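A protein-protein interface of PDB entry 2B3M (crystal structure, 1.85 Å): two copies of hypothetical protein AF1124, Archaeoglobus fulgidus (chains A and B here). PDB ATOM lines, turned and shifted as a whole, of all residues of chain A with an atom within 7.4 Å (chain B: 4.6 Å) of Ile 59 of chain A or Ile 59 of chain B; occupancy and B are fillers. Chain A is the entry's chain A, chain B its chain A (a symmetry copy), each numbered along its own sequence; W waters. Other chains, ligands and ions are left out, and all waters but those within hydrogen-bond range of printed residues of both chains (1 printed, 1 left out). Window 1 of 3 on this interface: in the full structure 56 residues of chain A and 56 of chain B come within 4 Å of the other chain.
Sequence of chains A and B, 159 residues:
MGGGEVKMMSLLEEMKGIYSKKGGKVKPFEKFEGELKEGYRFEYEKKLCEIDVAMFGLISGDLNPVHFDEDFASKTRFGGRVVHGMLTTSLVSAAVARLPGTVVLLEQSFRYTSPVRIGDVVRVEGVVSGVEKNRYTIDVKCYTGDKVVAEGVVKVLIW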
ATOM      1  N   TYR A  19       9.974 -22.674  10.942  1.00  0.00           N
ATOM      2  CA  TYR A  19      10.515 -21.702   9.991  1.00  0.00           C
ATOM      3  C   TYR A  19       9.496 -21.288   8.922  1.00  0.00           C
ATOM      4  O   TYR A  19       9.280 -20.082   8.688  1.00  0.00           O
ATOM      5  CB  TYR A  19      11.770 -22.291   9.329  1.00  0.00           C
ATOM      6  CG  TYR A  19      12.444 -21.428   8.286  1.00  0.00           C
ATOM      7  CD1 TYR A  19      13.078 -20.238   8.642  1.00  0.00           C
ATOM      8  CD2 TYR A  19      12.464 -21.815   6.945  1.00  0.00           C
ATOM      9  CE1 TYR A  19      13.731 -19.459   7.695  1.00  0.00           C
ATOM     10  CE2 TYR A  19      13.111 -21.036   5.978  1.00  0.00           C
ATOM     11  CZ  TYR A  19      13.728 -19.851   6.364  1.00  0.00           C
ATOM     12  OH  TYR A  19      14.351 -19.064   5.432  1.00  0.00           O
ATOM     13  N   LYS A  25      11.264 -19.185   3.580  1.00  0.00           N
ATOM     14  CA  LYS A  25      11.153 -19.908   2.309  1.00  0.00           C
ATOM     15  C   LYS A  25      12.073 -21.110   2.348  1.00  0.00           C
ATOM     16  O   LYS A  25      13.277 -20.946   2.338  1.00  0.00           O
ATOM     17  CB  LYS A  25      11.575 -19.010   1.138  1.00  0.00           C
ATOM     18  CG  LYS A  25      11.126 -17.551   1.246  1.00  0.00           C
ATOM     19  CD  LYS A  25       9.710 -17.323   0.742  1.00  0.00           C
ATOM     20  CE  LYS A  25       9.103 -16.130   1.436  1.00  0.00           C
ATOM     21  NZ  LYS A  25       7.733 -15.815   0.937  1.00  0.00           N
ATOM     22  N   LYS A  27      14.166 -23.692   0.798  1.00  0.00           N
ATOM     23  CA  LYS A  27      14.798 -23.954  -0.493  1.00  0.00           C
ATOM     24  C   LYS A  27      15.156 -25.438  -0.621  1.00  0.00           C
ATOM     25  O   LYS A  27      15.967 -25.942   0.154  1.00  0.00           O
ATOM     26  CB  LYS A  27      16.046 -23.074  -0.642  1.00  0.00           C
ATOM     27  CG  LYS A  27      15.765 -21.673  -1.170  1.00  0.00           C
ATOM     28  CD  LYS A  27      16.243 -21.585  -2.602  1.00  0.00           C
ATOM     29  CE  LYS A  27      15.286 -20.828  -3.454  1.00  0.00           C
ATOM     30  NZ  LYS A  27      15.800 -20.801  -4.842  1.00  0.00           N
ATOM     31  N   TYR A  44      21.580 -18.691  -8.018  1.00  0.00           N
ATOM     32  CA  TYR A  44      20.808 -19.172  -6.896  1.00  0.00           C
ATOM     33  C   TYR A  44      20.202 -17.935  -6.246  1.00  0.00           C
ATOM     34  O   TYR A  44      20.889 -16.924  -6.095  1.00  0.00           O
ATOM     35  CB  TYR A  44      21.757 -19.836  -5.897  1.00  0.00           C
ATOM     36  CG  TYR A  44      21.157 -20.212  -4.567  1.00  0.00           C
ATOM     37  CD1 TYR A  44      20.339 -21.331  -4.449  1.00  0.00           C
ATOM     38  CD2 TYR A  44      21.424 -19.464  -3.416  1.00  0.00           C
ATOM     39  CE1 TYR A  44      19.785 -21.702  -3.232  1.00  0.00           C
ATOM     40  CE2 TYR A  44      20.859 -19.835  -2.168  1.00  0.00           C
ATOM     41  CZ  TYR A  44      20.056 -20.965  -2.092  1.00  0.00           C
ATOM     42  OH  TYR A  44      19.485 -21.375  -0.905  1.00  0.00           O
ATOM     43  N   LYS A  46      17.301 -16.358  -3.036  1.00  0.00           N
ATOM     44  CA  LYS A  46      16.441 -16.614  -1.897  1.00  0.00           C
ATOM     45  C   LYS A  46      16.010 -15.282  -1.295  1.00  0.00           C
ATOM     46  O   LYS A  46      16.827 -14.359  -1.232  1.00  0.00           O
ATOM     47  CB  LYS A  46      17.218 -17.407  -0.841  1.00  0.00           C
ATOM     48  CG  LYS A  46      16.356 -18.043   0.258  1.00  0.00           C
ATOM     49  CD  LYS A  46      17.254 -18.993   1.091  1.00  0.00           C
ATOM     50  CE  LYS A  46      16.427 -19.763   2.118  1.00  0.00           C
ATOM     51  NZ  LYS A  46      15.918 -18.837   3.168  1.00  0.00           N
ATOM     52  N   LYS A  47      14.764 -15.217  -0.826  1.00  0.00           N
ATOM     53  CA  LYS A  47      14.277 -14.037  -0.077  1.00  0.00           C
ATOM     54  C   LYS A  47      14.808 -14.102   1.361  1.00  0.00           C
ATOM     55  O   LYS A  47      14.906 -15.191   1.970  1.00  0.00           O
ATOM     56  CB  LYS A  47      12.750 -14.010  -0.086  1.00  0.00           C
ATOM     57  CG  LYS A  47      12.066 -12.696   0.341  1.00  0.00           C
ATOM     58  CD  LYS A  47      10.557 -12.864   0.165  1.00  0.00           C
ATOM     59  CE  LYS A  47       9.853 -11.544  -0.075  1.00  0.00           C
ATOM     60  NZ  LYS A  47       8.479 -11.826  -0.528  1.00  0.00           N
ATOM     61  N   LEU A  48      15.192 -12.948   1.902  1.00  0.00           N
ATOM     62  CA  LEU A  48      15.628 -12.894   3.287  1.00  0.00           C
ATOM     63  C   LEU A  48      14.632 -12.066   4.083  1.00  0.00           C
ATOM     64  O   LEU A  48      14.560 -10.849   3.896  1.00  0.00           O
ATOM     65  CB  LEU A  48      17.047 -12.320   3.386  1.00  0.00           C
ATOM     66  CG  LEU A  48      18.115 -13.230   2.721  1.00  0.00           C
ATOM     67  CD1 LEU A  48      19.425 -12.489   2.643  1.00  0.00           C
ATOM     68  CD2 LEU A  48      18.264 -14.535   3.500  1.00  0.00           C
ATOM     69  N   CYS A  49      13.868 -12.734   4.948  1.00  0.00           N
ATOM     70  CA  CYS A  49      12.772 -12.098   5.687  1.00  0.00           C
ATOM     71  C   CYS A  49      13.142 -11.915   7.149  1.00  0.00           C
ATOM     72  O   CYS A  49      14.254 -12.274   7.555  1.00  0.00           O
ATOM     73  CB  CYS A  49      11.531 -12.990   5.594  1.00  0.00           C
ATOM     74  SG  CYS A  49      10.975 -13.205   3.891  1.00  0.00           S
ATOM     75  N   ILE A  51      12.315 -13.546   9.784  1.00  0.00           N
ATOM     76  CA  ILE A  51      12.699 -14.810  10.438  1.00  0.00           C
ATOM     77  C   ILE A  51      14.163 -15.158  10.157  1.00  0.00           C
ATOM     78  O   ILE A  51      14.878 -15.657  11.037  1.00  0.00           O
ATOM     79  CB  ILE A  51      11.727 -15.983  10.089  1.00  0.00           C
ATOM     80  CG1 ILE A  51      12.056 -17.270  10.873  1.00  0.00           C
ATOM     81  CG2 ILE A  51      11.672 -16.278   8.582  1.00  0.00           C
ATOM     82  CD1 ILE A  51      12.078 -17.119  12.377  1.00  0.00           C
ATOM     83  N   ASP A  52      14.614 -14.901   8.938  1.00  0.00           N
ATOM     84  CA  ASP A  52      16.014 -15.204   8.568  1.00  0.00           C
ATOM     85  C   ASP A  52      16.971 -14.339   9.354  1.00  0.00           C
ATOM     86  O   ASP A  52      18.003 -14.794   9.837  1.00  0.00           O
ATOM     87  CB  ASP A  52      16.215 -14.996   7.077  1.00  0.00           C
ATOM     88  CG  ASP A  52      15.317 -15.891   6.259  1.00  0.00           C
ATOM     89  OD1 ASP A  52      15.532 -17.132   6.277  1.00  0.00           O
ATOM     90  OD2 ASP A  52      14.374 -15.385   5.622  1.00  0.00           O
ATOM     91  N   VAL A  53      16.619 -13.057   9.489  1.00  0.00           N
ATOM     92  CA  VAL A  53      17.438 -12.148  10.254  1.00  0.00           C
ATOM     93  C   VAL A  53      17.457 -12.536  11.730  1.00  0.00           C
ATOM     94  O   VAL A  53      18.534 -12.513  12.339  1.00  0.00           O
ATOM     95  CB  VAL A  53      16.885 -10.687  10.091  1.00  0.00           C
ATOM     96  CG1 VAL A  53      17.737  -9.685  10.900  1.00  0.00           C
ATOM     97  CG2 VAL A  53      16.888 -10.345   8.602  1.00  0.00           C
ATOM     98  N   ALA A  54      16.281 -12.833  12.306  1.00  0.00           N
ATOM     99  CA  ALA A  54      16.173 -13.255  13.711  1.00  0.00           C
ATOM    100  C   ALA A  54      17.022 -14.501  13.960  1.00  0.00           C
ATOM    101  O   ALA A  54      17.754 -14.580  14.958  1.00  0.00           O
ATOM    102  CB  ALA A  54      14.749 -13.544  14.076  1.00  0.00           C
ATOM    103  N   MET A  55      16.882 -15.484  13.073  1.00  0.00           N
ATOM    104  CA  MET A  55      17.624 -16.769  13.246  1.00  0.00           C
ATOM    105  C   MET A  55      19.138 -16.521  13.140  1.00  0.00           C
ATOM    106  O   MET A  55      19.937 -17.062  13.940  1.00  0.00           O
ATOM    107  CB  MET A  55      17.155 -17.850  12.249  1.00  0.00           C
ATOM    108  CG  MET A  55      15.780 -18.477  12.542  1.00  0.00           C
ATOM    109  SD  MET A  55      15.426 -19.935  11.501  1.00  0.00           S
ATOM    110  CE  MET A  55      14.047 -20.681  12.377  1.00  0.00           C
ATOM    111  N   PHE A  56      19.541 -15.689  12.180  1.00  0.00           N
ATOM    112  CA  PHE A  56      20.958 -15.363  12.022  1.00  0.00           C
ATOM    113  C   PHE A  56      21.489 -14.684  13.277  1.00  0.00           C
ATOM    114  O   PHE A  56      22.572 -15.030  13.776  1.00  0.00           O
ATOM    115  CB  PHE A  56      21.199 -14.437  10.820  1.00  0.00           C
ATOM    116  CG  PHE A  56      22.636 -14.268  10.491  1.00  0.00           C
ATOM    117  CD1 PHE A  56      23.307 -15.238   9.733  1.00  0.00           C
ATOM    118  CD2 PHE A  56      23.350 -13.169  10.974  1.00  0.00           C
ATOM    119  CE1 PHE A  56      24.646 -15.082   9.417  1.00  0.00           C
ATOM    120  CE2 PHE A  56      24.708 -13.026  10.686  1.00  0.00           C
ATOM    121  CZ  PHE A  56      25.343 -13.959   9.886  1.00  0.00           C
ATOM    122  N   GLY A  57      20.726 -13.724  13.802  1.00  0.00           N
ATOM    123  CA  GLY A  57      21.079 -13.088  15.077  1.00  0.00           C
ATOM    124  C   GLY A  57      21.231 -14.077  16.229  1.00  0.00           C
ATOM    125  O   GLY A  57      22.155 -13.951  17.050  1.00  0.00           O
ATOM    126  N   LEU A  58      20.313 -15.043  16.329  1.00  0.00           N
ATOM    127  CA  LEU A  58      20.393 -16.020  17.412  1.00  0.00           C
ATOM    128  C   LEU A  58      21.619 -16.900  17.283  1.00  0.00           C
ATOM    129  O   LEU A  58      22.333 -17.150  18.274  1.00  0.00           O
ATOM    130  CB  LEU A  58      19.133 -16.895  17.486  1.00  0.00           C
ATOM    131  CG  LEU A  58      17.878 -16.141  17.949  1.00  0.00           C
ATOM    132  CD1 LEU A  58      16.640 -17.028  17.842  1.00  0.00           C
ATOM    133  CD2 LEU A  58      18.068 -15.611  19.371  1.00  0.00           C
ATOM    134  N   ILE A  59      21.842 -17.415  16.088  1.00  0.00           N
ATOM    135  CA  ILE A  59      22.904 -18.450  15.954  1.00  0.00           C
ATOM    136  C   ILE A  59      24.303 -17.816  16.025  1.00  0.00           C
ATOM    137  O   ILE A  59      25.241 -18.441  16.517  1.00  0.00           O
ATOM    138  CB  ILE A  59      22.729 -19.322  14.671  1.00  0.00           C
ATOM    139  CG1 ILE A  59      23.000 -18.524  13.408  1.00  0.00           C
ATOM    140  CG2 ILE A  59      21.343 -19.993  14.680  1.00  0.00           C
ATOM    141  CD1 ILE A  59      22.561 -19.209  12.092  1.00  0.00           C
ATOM    142  N   SER A  60      24.434 -16.579  15.526  1.00  0.00           N
ATOM    143  CA  SER A  60      25.717 -15.870  15.568  1.00  0.00           C
ATOM    144  C   SER A  60      25.932 -15.093  16.862  1.00  0.00           C
ATOM    145  O   SER A  60      27.074 -14.891  17.274  1.00  0.00           O
ATOM    146  CB  SER A  60      25.853 -14.890  14.411  1.00  0.00           C
ATOM    147  OG  SER A  60      24.862 -13.863  14.506  1.00  0.00           O
ATOM    148  N   GLY A  61      24.833 -14.672  17.484  1.00  0.00           N
ATOM    149  CA  GLY A  61      24.861 -13.695  18.584  1.00  0.00           C
ATOM    150  C   GLY A  61      24.901 -12.243  18.090  1.00  0.00           C
ATOM    151  O   GLY A  61      25.066 -11.325  18.897  1.00  0.00           O
ATOM    152  N   ASP A  62      24.773 -12.039  16.785  1.00  0.00           N
ATOM    153  CA  ASP A  62      24.798 -10.663  16.207  1.00  0.00           C
ATOM    154  C   ASP A  62      23.404 -10.033  16.295  1.00  0.00           C
ATOM    155  O   ASP A  62      22.587 -10.160  15.390  1.00  0.00           O
ATOM    156  CB  ASP A  62      25.337 -10.609  14.767  1.00  0.00           C
ATOM    157  CG  ASP A  62      25.534  -9.166  14.271  1.00  0.00           C
ATOM    158  OD1 ASP A  62      24.936  -8.265  14.915  1.00  0.00           O
ATOM    159  OD2 ASP A  62      26.240  -8.935  13.253  1.00  0.00           O
ATOM    160  N   LEU A  63      23.154  -9.355  17.397  1.00  0.00           N
ATOM    161  CA  LEU A  63      21.875  -8.669  17.597  1.00  0.00           C
ATOM    162  C   LEU A  63      22.041  -7.148  17.436  1.00  0.00           C
ATOM    163  O   LEU A  63      21.387  -6.352  18.131  1.00  0.00           O
ATOM    164  CB  LEU A  63      21.294  -9.045  18.961  1.00  0.00           C
ATOM    165  CG  LEU A  63      20.820 -10.491  19.180  1.00  0.00           C
ATOM    166  CD1 LEU A  63      20.122 -10.597  20.525  1.00  0.00           C
ATOM    167  CD2 LEU A  63      19.880 -10.951  18.054  1.00  0.00           C
ATOM    168  N   LEU A  87      24.719 -12.528   6.468  1.00  0.00           N
ATOM    169  CA  LEU A  87      23.531 -13.295   6.040  1.00  0.00           C
ATOM    170  C   LEU A  87      23.348 -13.304   4.511  1.00  0.00           C
ATOM    171  O   LEU A  87      23.143 -14.374   3.880  1.00  0.00           O
ATOM    172  CB  LEU A  87      22.242 -12.858   6.765  1.00  0.00           C
ATOM    173  CG  LEU A  87      20.918 -13.549   6.400  1.00  0.00           C
ATOM    174  CD1 LEU A  87      21.010 -15.072   6.539  1.00  0.00           C
ATOM    175  CD2 LEU A  87      19.709 -12.975   7.265  1.00  0.00           C
ATOM    176  N   SER A  90      25.845 -15.629   3.079  1.00  0.00           N
ATOM    177  CA  SER A  90      25.568 -17.032   3.452  1.00  0.00           C
ATOM    178  C   SER A  90      24.896 -17.744   2.282  1.00  0.00           C
ATOM    179  O   SER A  90      24.982 -18.983   2.142  1.00  0.00           O
ATOM    180  CB  SER A  90      24.669 -17.122   4.694  1.00  0.00           C
ATOM    181  OG  SER A  90      23.304 -16.905   4.367  1.00  0.00           O
ATOM    182  N   LEU A  91      24.210 -16.972   1.424  1.00  0.00           N
ATOM    183  CA  LEU A  91      23.561 -17.566   0.246  1.00  0.00           C
ATOM    184  C   LEU A  91      24.610 -18.114  -0.738  1.00  0.00           C
ATOM    185  O   LEU A  91      24.303 -18.967  -1.569  1.00  0.00           O
ATOM    186  CB  LEU A  91      22.667 -16.564  -0.474  1.00  0.00           C
ATOM    187  CG  LEU A  91      21.481 -16.054   0.382  1.00  0.00           C
ATOM    188  CD1 LEU A  91      20.590 -15.116  -0.490  1.00  0.00           C
ATOM    189  CD2 LEU A  91      20.660 -17.177   0.946  1.00  0.00           C
ATOM    190  N   ALA A  94      25.299 -21.594   0.158  1.00  0.00           N
ATOM    191  CA  ALA A  94      24.228 -22.458  -0.355  1.00  0.00           C
ATOM    192  C   ALA A  94      24.355 -22.714  -1.853  1.00  0.00           C
ATOM    193  O   ALA A  94      24.056 -23.824  -2.338  1.00  0.00           O
ATOM    194  CB  ALA A  94      22.844 -21.871  -0.015  1.00  0.00           C
ATOM    195  N   TYR B  19      14.706 -21.554  20.352  1.00  0.00           N
ATOM    196  CA  TYR B  19      16.150 -21.754  20.213  1.00  0.00           C
ATOM    197  C   TYR B  19      16.796 -22.313  21.487  1.00  0.00           C
ATOM    198  O   TYR B  19      17.538 -23.315  21.432  1.00  0.00           O
ATOM    199  CB  TYR B  19      16.807 -20.420  19.825  1.00  0.00           C
ATOM    200  CG  TYR B  19      18.312 -20.436  19.671  1.00  0.00           C
ATOM    201  CD1 TYR B  19      18.919 -21.144  18.633  1.00  0.00           C
ATOM    202  CD2 TYR B  19      19.126 -19.725  20.554  1.00  0.00           C
ATOM    203  CE1 TYR B  19      20.297 -21.132  18.464  1.00  0.00           C
ATOM    204  CE2 TYR B  19      20.518 -19.710  20.401  1.00  0.00           C
ATOM    205  CZ  TYR B  19      21.093 -20.431  19.360  1.00  0.00           C
ATOM    206  OH  TYR B  19      22.453 -20.447  19.202  1.00  0.00           O
ATOM    207  N   LYS B  46      31.415 -18.517  21.128  1.00  0.00           N
ATOM    208  CA  LYS B  46      30.092 -19.110  21.187  1.00  0.00           C
ATOM    209  C   LYS B  46      30.189 -20.572  20.769  1.00  0.00           C
ATOM    210  O   LYS B  46      30.943 -20.885  19.843  1.00  0.00           O
ATOM    211  CB  LYS B  46      29.162 -18.377  20.216  1.00  0.00           C
ATOM    212  CG  LYS B  46      27.667 -18.659  20.411  1.00  0.00           C
ATOM    213  CD  LYS B  46      26.865 -17.671  19.525  1.00  0.00           C
ATOM    214  CE  LYS B  46      25.365 -17.806  19.777  1.00  0.00           C
ATOM    215  NZ  LYS B  46      24.876 -19.121  19.274  1.00  0.00           N
ATOM    216  N   LEU B  48      28.714 -23.798  18.831  1.00  0.00           N
ATOM    217  CA  LEU B  48      27.860 -24.015  17.676  1.00  0.00           C
ATOM    218  C   LEU B  48      27.327 -25.439  17.720  1.00  0.00           C
ATOM    219  O   LEU B  48      28.094 -26.386  17.525  1.00  0.00           O
ATOM    220  CB  LEU B  48      28.627 -23.740  16.376  1.00  0.00           C
ATOM    221  CG  LEU B  48      29.044 -22.252  16.226  1.00  0.00           C
ATOM    222  CD1 LEU B  48      29.992 -22.112  15.063  1.00  0.00           C
ATOM    223  CD2 LEU B  48      27.812 -21.367  16.041  1.00  0.00           C
ATOM    224  N   ASP B  52      22.132 -24.632  15.729  1.00  0.00           N
ATOM    225  CA  ASP B  52      22.776 -23.534  14.976  1.00  0.00           C
ATOM    226  C   ASP B  52      23.005 -23.938  13.538  1.00  0.00           C
ATOM    227  O   ASP B  52      22.784 -23.166  12.610  1.00  0.00           O
ATOM    228  CB  ASP B  52      24.090 -23.152  15.634  1.00  0.00           C
ATOM    229  CG  ASP B  52      23.891 -22.684  17.055  1.00  0.00           C
ATOM    230  OD1 ASP B  52      23.293 -21.592  17.247  1.00  0.00           O
ATOM    231  OD2 ASP B  52      24.289 -23.402  17.992  1.00  0.00           O
ATOM    232  N   MET B  55      19.546 -24.173  11.768  1.00  0.00           N
ATOM    233  CA  MET B  55      19.007 -22.809  11.484  1.00  0.00           C
ATOM    234  C   MET B  55      19.789 -22.163  10.328  1.00  0.00           C
ATOM    235  O   MET B  55      19.195 -21.542   9.416  1.00  0.00           O
ATOM    236  CB  MET B  55      19.005 -21.911  12.739  1.00  0.00           C
ATOM    237  CG  MET B  55      17.931 -22.238  13.792  1.00  0.00           C
ATOM    238  SD  MET B  55      17.803 -20.967  15.097  1.00  0.00           S
ATOM    239  CE  MET B  55      16.222 -21.373  15.847  1.00  0.00           C
ATOM    240  N   PHE B  56      21.112 -22.323  10.340  1.00  0.00           N
ATOM    241  CA  PHE B  56      21.940 -21.776   9.265  1.00  0.00           C
ATOM    242  C   PHE B  56      21.554 -22.398   7.930  1.00  0.00           C
ATOM    243  O   PHE B  56      21.399 -21.692   6.921  1.00  0.00           O
ATOM    244  CB  PHE B  56      23.435 -22.027   9.513  1.00  0.00           C
ATOM    245  CG  PHE B  56      24.315 -21.293   8.570  1.00  0.00           C
ATOM    246  CD1 PHE B  56      24.621 -19.943   8.792  1.00  0.00           C
ATOM    247  CD2 PHE B  56      24.807 -21.924   7.424  1.00  0.00           C
ATOM    248  CE1 PHE B  56      25.448 -19.257   7.917  1.00  0.00           C
ATOM    249  CE2 PHE B  56      25.612 -21.225   6.524  1.00  0.00           C
ATOM    250  CZ  PHE B  56      25.957 -19.910   6.786  1.00  0.00           C
ATOM    251  N   GLY B  57      21.384 -23.722   7.918  1.00  0.00           N
ATOM    252  CA  GLY B  57      20.894 -24.411   6.719  1.00  0.00           C
ATOM    253  C   GLY B  57      19.550 -23.885   6.220  1.00  0.00           C
ATOM    254  O   GLY B  57      19.345 -23.732   5.005  1.00  0.00           O
ATOM    255  N   LEU B  58      18.612 -23.642   7.140  1.00  0.00           N
ATOM    256  CA  LEU B  58      17.300 -23.145   6.734  1.00  0.00           C
ATOM    257  C   LEU B  58      17.388 -21.754   6.141  1.00  0.00           C
ATOM    258  O   LEU B  58      16.773 -21.464   5.095  1.00  0.00           O
ATOM    259  CB  LEU B  58      16.302 -23.149   7.901  1.00  0.00           C
ATOM    260  CG  LEU B  58      15.883 -24.553   8.357  1.00  0.00           C
ATOM    261  CD1 LEU B  58      15.022 -24.483   9.617  1.00  0.00           C
ATOM    262  CD2 LEU B  58      15.163 -25.289   7.226  1.00  0.00           C
ATOM    263  N   ILE B  59      18.099 -20.874   6.823  1.00  0.00           N
ATOM    264  CA  ILE B  59      18.046 -19.447   6.403  1.00  0.00           C
ATOM    265  C   ILE B  59      18.858 -19.220   5.117  1.00  0.00           C
ATOM    266  O   ILE B  59      18.504 -18.368   4.305  1.00  0.00           O
ATOM    267  CB  ILE B  59      18.483 -18.472   7.542  1.00  0.00           C
ATOM    268  CG1 ILE B  59      19.967 -18.588   7.841  1.00  0.00           C
ATOM    269  CG2 ILE B  59      17.595 -18.688   8.782  1.00  0.00           C
ATOM    270  CD1 ILE B  59      20.430 -17.894   9.144  1.00  0.00           C
ATOM    271  N   SER B  60      19.947 -19.983   4.946  1.00  0.00           N
ATOM    272  CA  SER B  60      20.778 -19.870   3.743  1.00  0.00           C
ATOM    273  C   SER B  60      20.297 -20.750   2.596  1.00  0.00           C
ATOM    274  O   SER B  60      20.523 -20.420   1.432  1.00  0.00           O
ATOM    275  CB  SER B  60      22.229 -20.231   4.028  1.00  0.00           C
ATOM    276  OG  SER B  60      22.334 -21.603   4.420  1.00  0.00           O
ATOM    277  N   GLY B  61      19.639 -21.854   2.939  1.00  0.00           N
ATOM    278  CA  GLY B  61      19.341 -22.937   1.988  1.00  0.00           C
ATOM    279  C   GLY B  61      20.506 -23.919   1.818  1.00  0.00           C
ATOM    280  O   GLY B  61      20.451 -24.796   0.951  1.00  0.00           O
ATOM    281  N   LEU B  87      29.072 -20.372   8.836  1.00  0.00           N
ATOM    282  CA  LEU B  87      28.538 -20.275  10.210  1.00  0.00           C
ATOM    283  C   LEU B  87      29.620 -19.916  11.244  1.00  0.00           C
ATOM    284  O   LEU B  87      29.447 -18.994  12.083  1.00  0.00           O
ATOM    285  CB  LEU B  87      27.738 -21.524  10.632  1.00  0.00           C
ATOM    286  CG  LEU B  87      27.146 -21.580  12.049  1.00  0.00           C
ATOM    287  CD1 LEU B  87      26.261 -20.367  12.346  1.00  0.00           C
ATOM    288  CD2 LEU B  87      26.345 -22.936  12.288  1.00  0.00           C
ATOM    289  N   LEU B  91      30.314 -15.643  13.477  1.00  0.00           N
ATOM    290  CA  LEU B  91      30.641 -15.174  14.831  1.00  0.00           C
ATOM    291  C   LEU B  91      31.487 -13.888  14.775  1.00  0.00           C
ATOM    292  O   LEU B  91      31.543 -13.133  15.744  1.00  0.00           O
ATOM    293  CB  LEU B  91      31.387 -16.234  15.634  1.00  0.00           C
ATOM    294  CG  LEU B  91      30.566 -17.525  15.879  1.00  0.00           C
ATOM    295  CD1 LEU B  91      31.393 -18.488  16.786  1.00  0.00           C
ATOM    296  CD2 LEU B  91      29.230 -17.241  16.501  1.00  0.00           C
HETATM  297  O   HOH W   1      15.752 -22.990   3.074  1.00  0.00           O
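NZ of Lys 46 of chain A is in hydrogen-bond range of O of Ile 59 of chain B (2.9 Å).
The backbone carbonyl oxygen (O) of Ile 59 of chain A sits at hydrogen-bond distance from the side-chain amino group (NZ) of Lys 46 of chain B, 2.9 Å away.
The side-chain hydroxyl (OH) of Tyr 44 of chain A sits at hydrogen-bond distance from the backbone carbonyl oxygen (O) of Ser 60 of chain B, 2.7 Å away.
OH of Tyr 19 of chain B is in hydrogen-bond range of O of Leu 58 of chain A, at 3.4 Å.
O of Leu 58 of chain B is in hydrogen-bond range of NZ of Lys 46 of chain A (3.4 Å).
The backbone carbonyl oxygen of Leu 58 of chain B is in hydrogen-bond range of the side-chain hydroxyl of Tyr 19 of chain A.
NZ of Lys 46 of chain B lies within hydrogen-bond range of O of Leu 58 of chain A (3.4 Å).
Among the printed residues, pairs that only touch across the chains: Ala 94 of chain A with Ser 60 of chain B, Ser 60 of chain A with Leu 91 of chain B, Leu 91 of chain A with Ser 60 of chain B, Tyr 44 of chain A with Gly 61 of chain B, Asp 52 of chain A with Ile 59 of chain B, Ile 59 of chain A with Asp 52 of chain B, Ser 90 of chain A with Ser 60 of chain B, Lys 46 of chain A with Ser 60 of chain B, Ser 60 of chain A with Lys 46 of chain B, Ile 59 of chain A with Met 55 of chain B, Met 55 of chain A with Ile 59 of chain B, Ala 94 of chain A with Gly 61 of chain B, Ser 90 of chain A with Phe 56 of chain B, Ile 59 of chain A with Tyr 19 of chain B, Tyr 19 of chain A with Ile 59 of chain B, Ile 59 of chain A with Phe 56 of chain B, Phe 56 of chain A with Ile 59 of chain B, Ile 59 of chain A with Ile 59 of chain B, Leu 87 of chain A with Ile 59 of chain B, Ile 59 of chain A with Leu 87 of chain B, Gly 61 of chain A with Lys 46 of chain B, Lys 46 of chain A with Gly 61 of chain B, Leu 48 of chain A with Ile 59 of chain B and Ile 59 of chain A with Leu 48 of chain B.
Lys 46 of chain A touches Ser 60 of chain B, and with the chains exchanged Ser 60 of chain A touches Lys 46 of chain B.
Ile 59 of chain A touches Leu 87 of chain B, and with the chains exchanged Leu 87 of chain A touches Ile 59 of chain B.
Of the 25 printed residues of chain A, 15 touch a printed residue of chain B.
Printed residues of chain A that touch a printed residue of chain B: Tyr 19, Tyr 44, Lys 46, Leu 48, Asp 52, Met 55, Phe 56, Leu 58, Ile 59, Ser 60, Gly 61, Leu 87, Ser 90, Leu 91 and Ala 94.
Among the printed residues, no Asp or Glu carboxylate lies within 4 Å of a Lys or Arg side-chain nitrogen of the other chain.
Water W1 lies within hydrogen-bond range of the backbone carbonyl oxygen of Leu 58 of chain B, the backbone NH of Lys 27 of chain A and the backbone carbonyl oxygen of Lys 25 of chain A.
Printed residues of chain B within 4 Å of Ile 59 of chain A: Tyr 19, Lys 46, Leu 48, Asp 52, Met 55, Phe 56, Ile 59 and Leu 87.
Ile 59 of chain B touches just these residues of chain A: Tyr 19, Lys 46, Leu 48, Asp 52, Met 55, Phe 56, Ile 59 and Leu 87.
Printed residues of chain B within 4 Å of Ser 60 of chain A: Lys 46 and Leu 91.
Of the printed residues of chain B, Leu 87 of chain A touches Ile 59.
Gly 57 of chain A touches none of the printed residues of chain B.
The backbone carbonyl oxygen (O) of Leu 87 of chain A sits at hydrogen-bond distance from the side-chain hydroxyl (OG) of Ser 90 of chain A, at 2.6 Å.
OH of Tyr 19 of chain A sits at hydrogen-bond distance from NZ of Lys 46 of chain A (2.8 Å).
OG of Ser 60 of chain A sits at hydrogen-bond distance from O of Phe 56 of chain A (2.7 Å).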
